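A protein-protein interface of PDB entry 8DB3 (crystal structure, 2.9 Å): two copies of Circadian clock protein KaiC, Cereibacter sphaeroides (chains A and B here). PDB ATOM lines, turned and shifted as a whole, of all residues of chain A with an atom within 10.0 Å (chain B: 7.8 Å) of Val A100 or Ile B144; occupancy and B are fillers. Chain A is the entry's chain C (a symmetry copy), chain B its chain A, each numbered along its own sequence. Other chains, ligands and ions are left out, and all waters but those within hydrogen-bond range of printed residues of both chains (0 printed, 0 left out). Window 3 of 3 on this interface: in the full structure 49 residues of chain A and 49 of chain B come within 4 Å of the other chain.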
ATOM      1  N   GLU A  62      10.179  17.361   0.866  1.00  0.00           N
ATOM      2  CA  GLU A  62       8.983  16.535   0.966  1.00  0.00           C
ATOM      3  C   GLU A  62       8.918  15.514  -0.168  1.00  0.00           C
ATOM      4  O   GLU A  62       8.813  14.310   0.081  1.00  0.00           O
ATOM      5  CB  GLU A  62       7.709  17.385   0.947  1.00  0.00           C
ATOM      6  CG  GLU A  62       7.845  18.769   1.540  1.00  0.00           C
ATOM      7  CD  GLU A  62       6.532  19.532   1.513  1.00  0.00           C
ATOM      8  OE1 GLU A  62       6.205  20.193   2.522  1.00  0.00           O
ATOM      9  OE2 GLU A  62       5.832  19.471   0.479  1.00  0.00           O
ATOM     10  N   VAL A  95      11.454  15.764   8.365  1.00  0.00           N
ATOM     11  CA  VAL A  95      11.387  16.263   9.734  1.00  0.00           C
ATOM     12  C   VAL A  95       9.998  15.974  10.287  1.00  0.00           C
ATOM     13  O   VAL A  95       9.098  15.542   9.566  1.00  0.00           O
ATOM     14  CB  VAL A  95      11.686  17.779   9.803  1.00  0.00           C
ATOM     15  CG1 VAL A  95      13.143  18.057   9.470  1.00  0.00           C
ATOM     16  CG2 VAL A  95      10.766  18.539   8.853  1.00  0.00           C
ATOM     17  N   ASP A  96       9.820  16.213  11.592  1.00  0.00           N
ATOM     18  CA  ASP A  96       8.481  16.212  12.182  1.00  0.00           C
ATOM     19  C   ASP A  96       8.519  16.769  13.607  1.00  0.00           C
ATOM     20  O   ASP A  96       7.950  17.845  13.838  1.00  0.00           O
ATOM     21  CB  ASP A  96       7.884  14.808  12.137  1.00  0.00           C
ATOM     22  CG  ASP A  96       6.416  14.787  12.527  1.00  0.00           C
ATOM     23  OD1 ASP A  96       6.022  15.601  13.391  1.00  0.00           O
ATOM     24  OD2 ASP A  96       5.661  13.958  11.980  1.00  0.00           O
ATOM     25  N   PRO A  97       9.150  16.109  14.590  1.00  0.00           N
ATOM     26  CA  PRO A  97       9.314  16.768  15.897  1.00  0.00           C
ATOM     27  C   PRO A  97      10.434  17.790  15.912  1.00  0.00           C
ATOM     28  O   PRO A  97      10.449  18.657  16.797  1.00  0.00           O
ATOM     29  CB  PRO A  97       9.617  15.604  16.847  1.00  0.00           C
ATOM     30  CG  PRO A  97      10.355  14.645  15.993  1.00  0.00           C
ATOM     31  CD  PRO A  97       9.700  14.738  14.621  1.00  0.00           C
ATOM     32  N   SER A  98      11.374  17.711  14.968  1.00  0.00           N
ATOM     33  CA  SER A  98      12.450  18.689  14.896  1.00  0.00           C
ATOM     34  C   SER A  98      11.948  20.067  14.498  1.00  0.00           C
ATOM     35  O   SER A  98      12.629  21.063  14.763  1.00  0.00           O
ATOM     36  CB  SER A  98      13.514  18.216  13.902  1.00  0.00           C
ATOM     37  OG  SER A  98      14.605  19.115  13.846  1.00  0.00           O
ATOM     38  N   GLU A  99      10.768  20.149  13.882  1.00  0.00           N
ATOM     39  CA  GLU A  99      10.306  21.425  13.354  1.00  0.00           C
ATOM     40  C   GLU A  99       9.932  22.402  14.463  1.00  0.00           C
ATOM     41  O   GLU A  99      10.065  23.615  14.281  1.00  0.00           O
ATOM     42  CB  GLU A  99       9.117  21.206  12.420  1.00  0.00           C
ATOM     43  CG  GLU A  99       9.508  20.887  10.982  1.00  0.00           C
ATOM     44  CD  GLU A  99      10.431  21.929  10.370  1.00  0.00           C
ATOM     45  OE1 GLU A  99      10.054  23.118  10.326  1.00  0.00           O
ATOM     46  OE2 GLU A  99      11.541  21.557   9.933  1.00  0.00           O
ATOM     47  N   VAL A 100       9.465  21.904  15.612  1.00  0.00           N
ATOM     48  CA  VAL A 100       9.101  22.804  16.704  1.00  0.00           C
ATOM     49  C   VAL A 100      10.261  23.736  17.031  1.00  0.00           C
ATOM     50  O   VAL A 100      10.071  24.932  17.280  1.00  0.00           O
ATOM     51  CB  VAL A 100       8.658  22.004  17.945  1.00  0.00           C
ATOM     52  CG1 VAL A 100       7.413  21.189  17.634  1.00  0.00           C
ATOM     53  CG2 VAL A 100       9.791  21.114  18.443  1.00  0.00           C
ATOM     54  N   ALA A 101      11.479  23.202  17.031  1.00  0.00           N
ATOM     55  CA  ALA A 101      12.668  23.986  17.339  1.00  0.00           C
ATOM     56  C   ALA A 101      13.441  24.312  16.064  1.00  0.00           C
ATOM     57  O   ALA A 101      14.569  24.804  16.114  1.00  0.00           O
ATOM     58  CB  ALA A 101      13.552  23.235  18.319  1.00  0.00           C
ATOM     59  N   GLU A 133      10.716  25.618   2.532  1.00  0.00           N
ATOM     60  CA  GLU A 133       9.654  26.023   3.456  1.00  0.00           C
ATOM     61  C   GLU A 133       9.430  24.985   4.546  1.00  0.00           C
ATOM     62  O   GLU A 133       9.077  25.342   5.672  1.00  0.00           O
ATOM     63  CB  GLU A 133       8.360  26.270   2.680  1.00  0.00           C
ATOM     64  CG  GLU A 133       8.350  27.573   1.893  1.00  0.00           C
ATOM     65  CD  GLU A 133       8.798  27.405   0.448  1.00  0.00           C
ATOM     66  OE1 GLU A 133       9.331  26.329   0.096  1.00  0.00           O
ATOM     67  OE2 GLU A 133       8.614  28.360  -0.338  1.00  0.00           O
ATOM     68  N   SER A 134       9.652  23.702   4.246  1.00  0.00           N
ATOM     69  CA  SER A 134       9.433  22.670   5.257  1.00  0.00           C
ATOM     70  C   SER A 134      10.308  22.912   6.482  1.00  0.00           C
ATOM     71  O   SER A 134       9.888  22.653   7.616  1.00  0.00           O
ATOM     72  CB  SER A 134       9.714  21.288   4.670  1.00  0.00           C
ATOM     73  OG  SER A 134       8.930  20.302   5.320  1.00  0.00           O
ATOM     74  N   LEU A 135      11.525  23.413   6.275  1.00  0.00           N
ATOM     75  CA  LEU A 135      12.417  23.722   7.384  1.00  0.00           C
ATOM     76  C   LEU A 135      12.167  25.112   7.952  1.00  0.00           C
ATOM     77  O   LEU A 135      12.236  25.303   9.171  1.00  0.00           O
ATOM     78  CB  LEU A 135      13.873  23.607   6.931  1.00  0.00           C
ATOM     79  CG  LEU A 135      14.933  23.543   8.031  1.00  0.00           C
ATOM     80  CD1 LEU A 135      15.938  22.443   7.712  1.00  0.00           C
ATOM     81  CD2 LEU A 135      15.635  24.879   8.195  1.00  0.00           C
ATOM     82  N   PHE A 136      11.862  26.087   7.099  1.00  0.00           N
ATOM     83  CA  PHE A 136      11.830  27.474   7.547  1.00  0.00           C
ATOM     84  C   PHE A 136      10.447  27.968   7.960  1.00  0.00           C
ATOM     85  O   PHE A 136      10.332  29.109   8.423  1.00  0.00           O
ATOM     86  CB  PHE A 136      12.396  28.386   6.456  1.00  0.00           C
ATOM     87  CG  PHE A 136      13.886  28.300   6.314  1.00  0.00           C
ATOM     88  CD1 PHE A 136      14.485  27.126   5.891  1.00  0.00           C
ATOM     89  CD2 PHE A 136      14.690  29.385   6.613  1.00  0.00           C
ATOM     90  CE1 PHE A 136      15.856  27.038   5.759  1.00  0.00           C
ATOM     91  CE2 PHE A 136      16.064  29.304   6.485  1.00  0.00           C
ATOM     92  CZ  PHE A 136      16.647  28.128   6.057  1.00  0.00           C
ATOM     93  N   SER A 137       9.401  27.152   7.825  1.00  0.00           N
ATOM     94  CA  SER A 137       8.087  27.557   8.309  1.00  0.00           C
ATOM     95  C   SER A 137       8.002  27.476   9.825  1.00  0.00           C
ATOM     96  O   SER A 137       7.074  28.042  10.417  1.00  0.00           O
ATOM     97  CB  SER A 137       7.002  26.686   7.679  1.00  0.00           C
ATOM     98  OG  SER A 137       7.240  25.313   7.928  1.00  0.00           O
ATOM     99  N   ALA A 138       8.945  26.780  10.461  1.00  0.00           N
ATOM    100  CA  ALA A 138       8.996  26.750  11.915  1.00  0.00           C
ATOM    101  C   ALA A 138       9.378  28.106  12.489  1.00  0.00           C
ATOM    102  O   ALA A 138       8.943  28.457  13.591  1.00  0.00           O
ATOM    103  CB  ALA A 138       9.992  25.686  12.378  1.00  0.00           C
ATOM    104  N   PHE A 139      10.190  28.873  11.765  1.00  0.00           N
ATOM    105  CA  PHE A 139      10.658  30.169  12.245  1.00  0.00           C
ATOM    106  C   PHE A 139       9.512  31.170  12.195  1.00  0.00           C
ATOM    107  O   PHE A 139       9.078  31.580  11.113  1.00  0.00           O
ATOM    108  CB  PHE A 139      11.843  30.633  11.408  1.00  0.00           C
ATOM    109  CG  PHE A 139      13.046  29.746  11.525  1.00  0.00           C
ATOM    110  CD1 PHE A 139      13.695  29.596  12.740  1.00  0.00           C
ATOM    111  CD2 PHE A 139      13.525  29.052  10.427  1.00  0.00           C
ATOM    112  CE1 PHE A 139      14.801  28.776  12.855  1.00  0.00           C
ATOM    113  CE2 PHE A 139      14.631  28.230  10.535  1.00  0.00           C
ATOM    114  CZ  PHE A 139      15.269  28.091  11.751  1.00  0.00           C
ATOM    115  N   SER A 140       9.021  31.563  13.369  1.00  0.00           N
ATOM    116  CA  SER A 140       7.884  32.467  13.469  1.00  0.00           C
ATOM    117  C   SER A 140       8.304  33.930  13.468  1.00  0.00           C
ATOM    118  O   SER A 140       7.667  34.753  12.801  1.00  0.00           O
ATOM    119  CB  SER A 140       7.084  32.158  14.737  1.00  0.00           C
ATOM    120  OG  SER A 140       6.438  30.902  14.632  1.00  0.00           O
ATOM    121  N   ASN A 141       9.357  34.273  14.196  1.00  0.00           N
ATOM    122  CA  ASN A 141       9.799  35.661  14.234  1.00  0.00           C
ATOM    123  C   ASN A 141      10.376  36.053  12.878  1.00  0.00           C
ATOM    124  O   ASN A 141      11.228  35.332  12.336  1.00  0.00           O
ATOM    125  CB  ASN A 141      10.837  35.881  15.325  1.00  0.00           C
ATOM    126  CG  ASN A 141      10.999  37.346  15.677  1.00  0.00           C
ATOM    127  OD1 ASN A 141      11.760  38.069  15.034  1.00  0.00           O
ATOM    128  ND2 ASN A 141      10.265  37.797  16.687  1.00  0.00           N
ATOM    129  N   PHE B 136      -6.453  17.835  11.154  1.00  0.00           N
ATOM    130  CA  PHE B 136      -5.455  18.826  10.770  1.00  0.00           C
ATOM    131  C   PHE B 136      -5.840  20.256  11.142  1.00  0.00           C
ATOM    132  O   PHE B 136      -5.030  21.161  10.917  1.00  0.00           O
ATOM    133  CB  PHE B 136      -5.188  18.733   9.262  1.00  0.00           C
ATOM    134  CG  PHE B 136      -4.576  17.420   8.836  1.00  0.00           C
ATOM    135  CD1 PHE B 136      -4.420  17.119   7.491  1.00  0.00           C
ATOM    136  CD2 PHE B 136      -4.155  16.492   9.775  1.00  0.00           C
ATOM    137  CE1 PHE B 136      -3.854  15.920   7.096  1.00  0.00           C
ATOM    138  CE2 PHE B 136      -3.596  15.295   9.386  1.00  0.00           C
ATOM    139  CZ  PHE B 136      -3.443  15.007   8.049  1.00  0.00           C
ATOM    140  N   ALA B 138      -6.293  21.142  14.246  1.00  0.00           N
ATOM    141  CA  ALA B 138      -5.732  21.342  15.574  1.00  0.00           C
ATOM    142  C   ALA B 138      -4.250  21.686  15.547  1.00  0.00           C
ATOM    143  O   ALA B 138      -3.713  22.132  16.567  1.00  0.00           O
ATOM    144  CB  ALA B 138      -5.945  20.087  16.430  1.00  0.00           C
ATOM    145  N   PHE B 139      -3.579  21.498  14.414  1.00  0.00           N
ATOM    146  CA  PHE B 139      -2.160  21.819  14.296  1.00  0.00           C
ATOM    147  C   PHE B 139      -2.020  23.306  13.989  1.00  0.00           C
ATOM    148  O   PHE B 139      -2.317  23.751  12.875  1.00  0.00           O
ATOM    149  CB  PHE B 139      -1.510  20.962  13.215  1.00  0.00           C
ATOM    150  CG  PHE B 139      -1.375  19.511  13.590  1.00  0.00           C
ATOM    151  CD1 PHE B 139      -0.660  19.133  14.716  1.00  0.00           C
ATOM    152  CD2 PHE B 139      -1.962  18.524  12.814  1.00  0.00           C
ATOM    153  CE1 PHE B 139      -0.535  17.797  15.059  1.00  0.00           C
ATOM    154  CE2 PHE B 139      -1.839  17.187  13.154  1.00  0.00           C
ATOM    155  CZ  PHE B 139      -1.125  16.825  14.277  1.00  0.00           C
ATOM    156  N   SER B 140      -1.569  24.077  14.979  1.00  0.00           N
ATOM    157  CA  SER B 140      -1.403  25.513  14.792  1.00  0.00           C
ATOM    158  C   SER B 140      -0.134  25.828  14.011  1.00  0.00           C
ATOM    159  O   SER B 140      -0.159  26.628  13.069  1.00  0.00           O
ATOM    160  CB  SER B 140      -1.380  26.216  16.151  1.00  0.00           C
ATOM    161  OG  SER B 140      -2.386  25.700  17.004  1.00  0.00           O
ATOM    162  N   ASN B 141       0.977  25.211  14.383  1.00  0.00           N
ATOM    163  CA  ASN B 141       2.264  25.504  13.752  1.00  0.00           C
ATOM    164  C   ASN B 141       2.259  25.034  12.305  1.00  0.00           C
ATOM    165  O   ASN B 141       2.002  23.848  12.048  1.00  0.00           O
ATOM    166  CB  ASN B 141       3.388  24.826  14.539  1.00  0.00           C
ATOM    167  CG  ASN B 141       4.770  25.264  14.085  1.00  0.00           C
ATOM    168  OD1 ASN B 141       5.033  25.390  12.889  1.00  0.00           O
ATOM    169  ND2 ASN B 141       5.664  25.488  15.042  1.00  0.00           N
ATOM    170  N   PRO B 142       2.535  25.913  11.333  1.00  0.00           N
ATOM    171  CA  PRO B 142       2.525  25.458   9.931  1.00  0.00           C
ATOM    172  C   PRO B 142       3.528  24.351   9.663  1.00  0.00           C
ATOM    173  O   PRO B 142       3.231  23.405   8.919  1.00  0.00           O
ATOM    174  CB  PRO B 142       2.865  26.730   9.135  1.00  0.00           C
ATOM    175  CG  PRO B 142       2.675  27.871  10.085  1.00  0.00           C
ATOM    176  CD  PRO B 142       2.927  27.329  11.458  1.00  0.00           C
ATOM    177  N   ALA B 143       4.725  24.458  10.244  1.00  0.00           N
ATOM    178  CA  ALA B 143       5.735  23.424  10.056  1.00  0.00           C
ATOM    179  C   ALA B 143       5.227  22.076  10.547  1.00  0.00           C
ATOM    180  O   ALA B 143       5.343  21.064   9.849  1.00  0.00           O
ATOM    181  CB  ALA B 143       7.023  23.818  10.780  1.00  0.00           C
ATOM    182  N   ILE B 144       4.649  22.048  11.751  1.00  0.00           N
ATOM    183  CA  ILE B 144       4.096  20.808  12.290  1.00  0.00           C
ATOM    184  C   ILE B 144       3.014  20.265  11.365  1.00  0.00           C
ATOM    185  O   ILE B 144       2.986  19.069  11.044  1.00  0.00           O
ATOM    186  CB  ILE B 144       3.541  21.046  13.707  1.00  0.00           C
ATOM    187  CG1 ILE B 144       4.636  20.878  14.756  1.00  0.00           C
ATOM    188  CG2 ILE B 144       2.383  20.093  13.998  1.00  0.00           C
ATOM    189  CD1 ILE B 144       4.403  21.721  15.988  1.00  0.00           C
ATOM    190  N   LEU B 145       2.077  21.125  10.968  1.00  0.00           N
ATOM    191  CA  LEU B 145       0.950  20.653  10.173  1.00  0.00           C
ATOM    192  C   LEU B 145       1.434  20.027   8.873  1.00  0.00           C
ATOM    193  O   LEU B 145       0.995  18.936   8.491  1.00  0.00           O
ATOM    194  CB  LEU B 145      -0.018  21.798   9.888  1.00  0.00           C
ATOM    195  CG  LEU B 145      -1.186  21.436   8.971  1.00  0.00           C
ATOM    196  CD1 LEU B 145      -2.045  20.340   9.577  1.00  0.00           C
ATOM    197  CD2 LEU B 145      -2.025  22.669   8.683  1.00  0.00           C
ATOM    198  N   ARG B 146       2.345  20.707   8.174  1.00  0.00           N
ATOM    199  CA  ARG B 146       2.812  20.165   6.904  1.00  0.00           C
ATOM    200  C   ARG B 146       3.686  18.937   7.115  1.00  0.00           C
ATOM    201  O   ARG B 146       3.688  18.037   6.273  1.00  0.00           O
ATOM    202  CB  ARG B 146       3.553  21.238   6.110  1.00  0.00           C
ATOM    203  CG  ARG B 146       4.992  21.452   6.514  1.00  0.00           C
ATOM    204  CD  ARG B 146       5.653  22.505   5.616  1.00  0.00           C
ATOM    205  NE  ARG B 146       5.351  22.301   4.203  1.00  0.00           N
ATOM    206  CZ  ARG B 146       4.945  23.254   3.371  1.00  0.00           C
ATOM    207  NH1 ARG B 146       4.785  24.504   3.773  1.00  0.00           N
ATOM    208  NH2 ARG B 146       4.694  22.941   2.103  1.00  0.00           N
ATOM    209  N   ALA B 147       4.414  18.860   8.231  1.00  0.00           N
ATOM    210  CA  ALA B 147       5.182  17.653   8.511  1.00  0.00           C
ATOM    211  C   ALA B 147       4.259  16.455   8.692  1.00  0.00           C
ATOM    212  O   ALA B 147       4.532  15.366   8.177  1.00  0.00           O
ATOM    213  CB  ALA B 147       6.051  17.854   9.751  1.00  0.00           C
ATOM    214  N   GLU B 148       3.151  16.642   9.414  1.00  0.00           N
ATOM    215  CA  GLU B 148       2.197  15.551   9.587  1.00  0.00           C
ATOM    216  C   GLU B 148       1.528  15.196   8.263  1.00  0.00           C
ATOM    217  O   GLU B 148       1.330  14.012   7.953  1.00  0.00           O
ATOM    218  CB  GLU B 148       1.142  15.925  10.631  1.00  0.00           C
ATOM    219  CG  GLU B 148       1.707  16.382  11.969  1.00  0.00           C
ATOM    220  CD  GLU B 148       1.982  15.231  12.922  1.00  0.00           C
ATOM    221  OE1 GLU B 148       1.661  14.073  12.579  1.00  0.00           O
ATOM    222  OE2 GLU B 148       2.521  15.490  14.019  1.00  0.00           O
ATOM    223  N   ILE B 149       1.158  16.211   7.476  1.00  0.00           N
ATOM    224  CA  ILE B 149       0.590  15.955   6.158  1.00  0.00           C
ATOM    225  C   ILE B 149       1.556  15.127   5.324  1.00  0.00           C
ATOM    226  O   ILE B 149       1.159  14.176   4.639  1.00  0.00           O
ATOM    227  CB  ILE B 149       0.243  17.280   5.456  1.00  0.00           C
ATOM    228  CG1 ILE B 149      -0.900  17.988   6.180  1.00  0.00           C
ATOM    229  CG2 ILE B 149      -0.116  17.029   3.996  1.00  0.00           C
ATOM    230  CD1 ILE B 149      -1.023  19.454   5.824  1.00  0.00           C
ATOM    231  N   ARG B 150       2.840  15.485   5.362  1.00  0.00           N
ATOM    232  CA  ARG B 150       3.839  14.741   4.611  1.00  0.00           C
ATOM    233  C   ARG B 150       3.965  13.323   5.140  1.00  0.00           C
ATOM    234  O   ARG B 150       4.102  12.385   4.365  1.00  0.00           O
ATOM    235  CB  ARG B 150       5.191  15.453   4.669  1.00  0.00           C
ATOM    236  CG  ARG B 150       6.236  14.861   3.730  1.00  0.00           C
ATOM    237  CD  ARG B 150       7.615  14.794   4.388  1.00  0.00           C
ATOM    238  NE  ARG B 150       7.860  15.936   5.261  1.00  0.00           N
ATOM    239  CZ  ARG B 150       8.357  15.857   6.489  1.00  0.00           C
ATOM    240  NH1 ARG B 150       8.713  14.700   7.018  1.00  0.00           N
ATOM    241  NH2 ARG B 150       8.501  16.971   7.200  1.00  0.00           N
ATOM    242  N   ARG B 151       3.936  13.146   6.458  1.00  0.00           N
ATOM    243  CA  ARG B 151       3.987  11.795   7.007  1.00  0.00           C
ATOM    244  C   ARG B 151       2.849  10.950   6.444  1.00  0.00           C
ATOM    245  O   ARG B 151       3.057   9.811   6.012  1.00  0.00           O
ATOM    246  CB  ARG B 151       3.928  11.838   8.532  1.00  0.00           C
ATOM    247  CG  ARG B 151       4.434  10.563   9.194  1.00  0.00           C
ATOM    248  CD  ARG B 151       5.204  10.857  10.473  1.00  0.00           C
ATOM    249  NE  ARG B 151       4.319  11.251  11.564  1.00  0.00           N
ATOM    250  CZ  ARG B 151       4.683  11.328  12.836  1.00  0.00           C
ATOM    251  NH1 ARG B 151       5.916  11.047  13.221  1.00  0.00           N
ATOM    252  NH2 ARG B 151       3.786  11.698  13.745  1.00  0.00           N
ATOM    253  N   LEU B 179      -1.456  24.381   2.492  1.00  0.00           N
ATOM    254  CA  LEU B 179      -0.270  23.532   2.467  1.00  0.00           C
ATOM    255  C   LEU B 179      -0.479  22.211   1.748  1.00  0.00           C
ATOM    256  O   LEU B 179       0.427  21.745   1.046  1.00  0.00           O
ATOM    257  CB  LEU B 179       0.198  23.241   3.900  1.00  0.00           C
ATOM    258  CG  LEU B 179       0.371  24.451   4.815  1.00  0.00           C
ATOM    259  CD1 LEU B 179       0.253  24.023   6.271  1.00  0.00           C
ATOM    260  CD2 LEU B 179       1.703  25.133   4.553  1.00  0.00           C
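Hydrophobic or aromatic side chains of chain A within 4 Å of the printed part of chain B: Val A95, Val A100 and Ala A138.
Of the 16 printed residues of chain B, 7 touch a printed residue of chain A.
Hydrophobic or aromatic side chains of chain B that line the printed part of chain A: Ala B143, Ile B144 and Ala B147.
Among the printed residues, Asp or Glu carboxylates within 4 Å of a Lys or Arg side-chain nitrogen of the other chain: Glu A62 with Arg B146 (2.8 Å) and Asp A96 with Arg B151 (3.0 Å).
Among the printed residues, merely in contact across the chains: Glu A99 with Ala B143, Ser A137 with Ala B143, Val A100 with Ile B144, Ala A138 with Ala B143, Asp A96 with Glu B148, Ser A134 with Arg B146, Asp A96 with Ala B147, Val A95 with Ala B147, Ser A134 with Arg B150 and Ser A137 with Arg B146.
5 positions are printed for both chains.
Printed residues of chain B within 4 Å of Glu A99: Ala B143 (3.1 Å).
Val A100 touches just one residue of chain B: Ile B144 (3.5 Å).
Asn B141 touches none of the printed residues of chain A.
Ala B143 touches just these residues of chain A: Glu A99 (3.1 Å), Ser A137 (3.2 Å) and Ala A138 (3.5 Å).
Of chain A, only Val A100 (3.5 Å) comes within 4 Å of Ile B144.
Printed residues of chain A within 4 Å of Glu B148: Asp A96.
Of the printed residues of chain A, Arg B150 touches Val A95 and Ser A134.
The nearest residue of chain B that does not touch Val A100 is Asn B141 (4.7 Å).
The nearest printed residue of chain B that does not touch Glu A62 is Arg B150 (4.04 Å).
O of Glu A133 lies within hydrogen-bond range of OG of Ser A137.
The side-chain amide oxygen of Asn B141 sits at hydrogen-bond distance from the backbone NH of Ala B143, 2.8 Å away.
NH2 of Arg B151 is in salt-bridge range of OE1 of Glu B148 (3.4 Å).
The backbone carbonyl oxygen of Val A95 sits at hydrogen-bond distance from the guanidinium group of Arg B150 (2.7 Å).
The guanidinium group (NE) of Arg B146 is in salt-bridge range of the side-chain carboxylate (OE1) of Glu A62 (2.8 Å).
The guanidinium group (NE) of Arg B151 lies within salt-bridge range of the side-chain carboxylate (OD2) of Asp A96 (3.0 Å).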
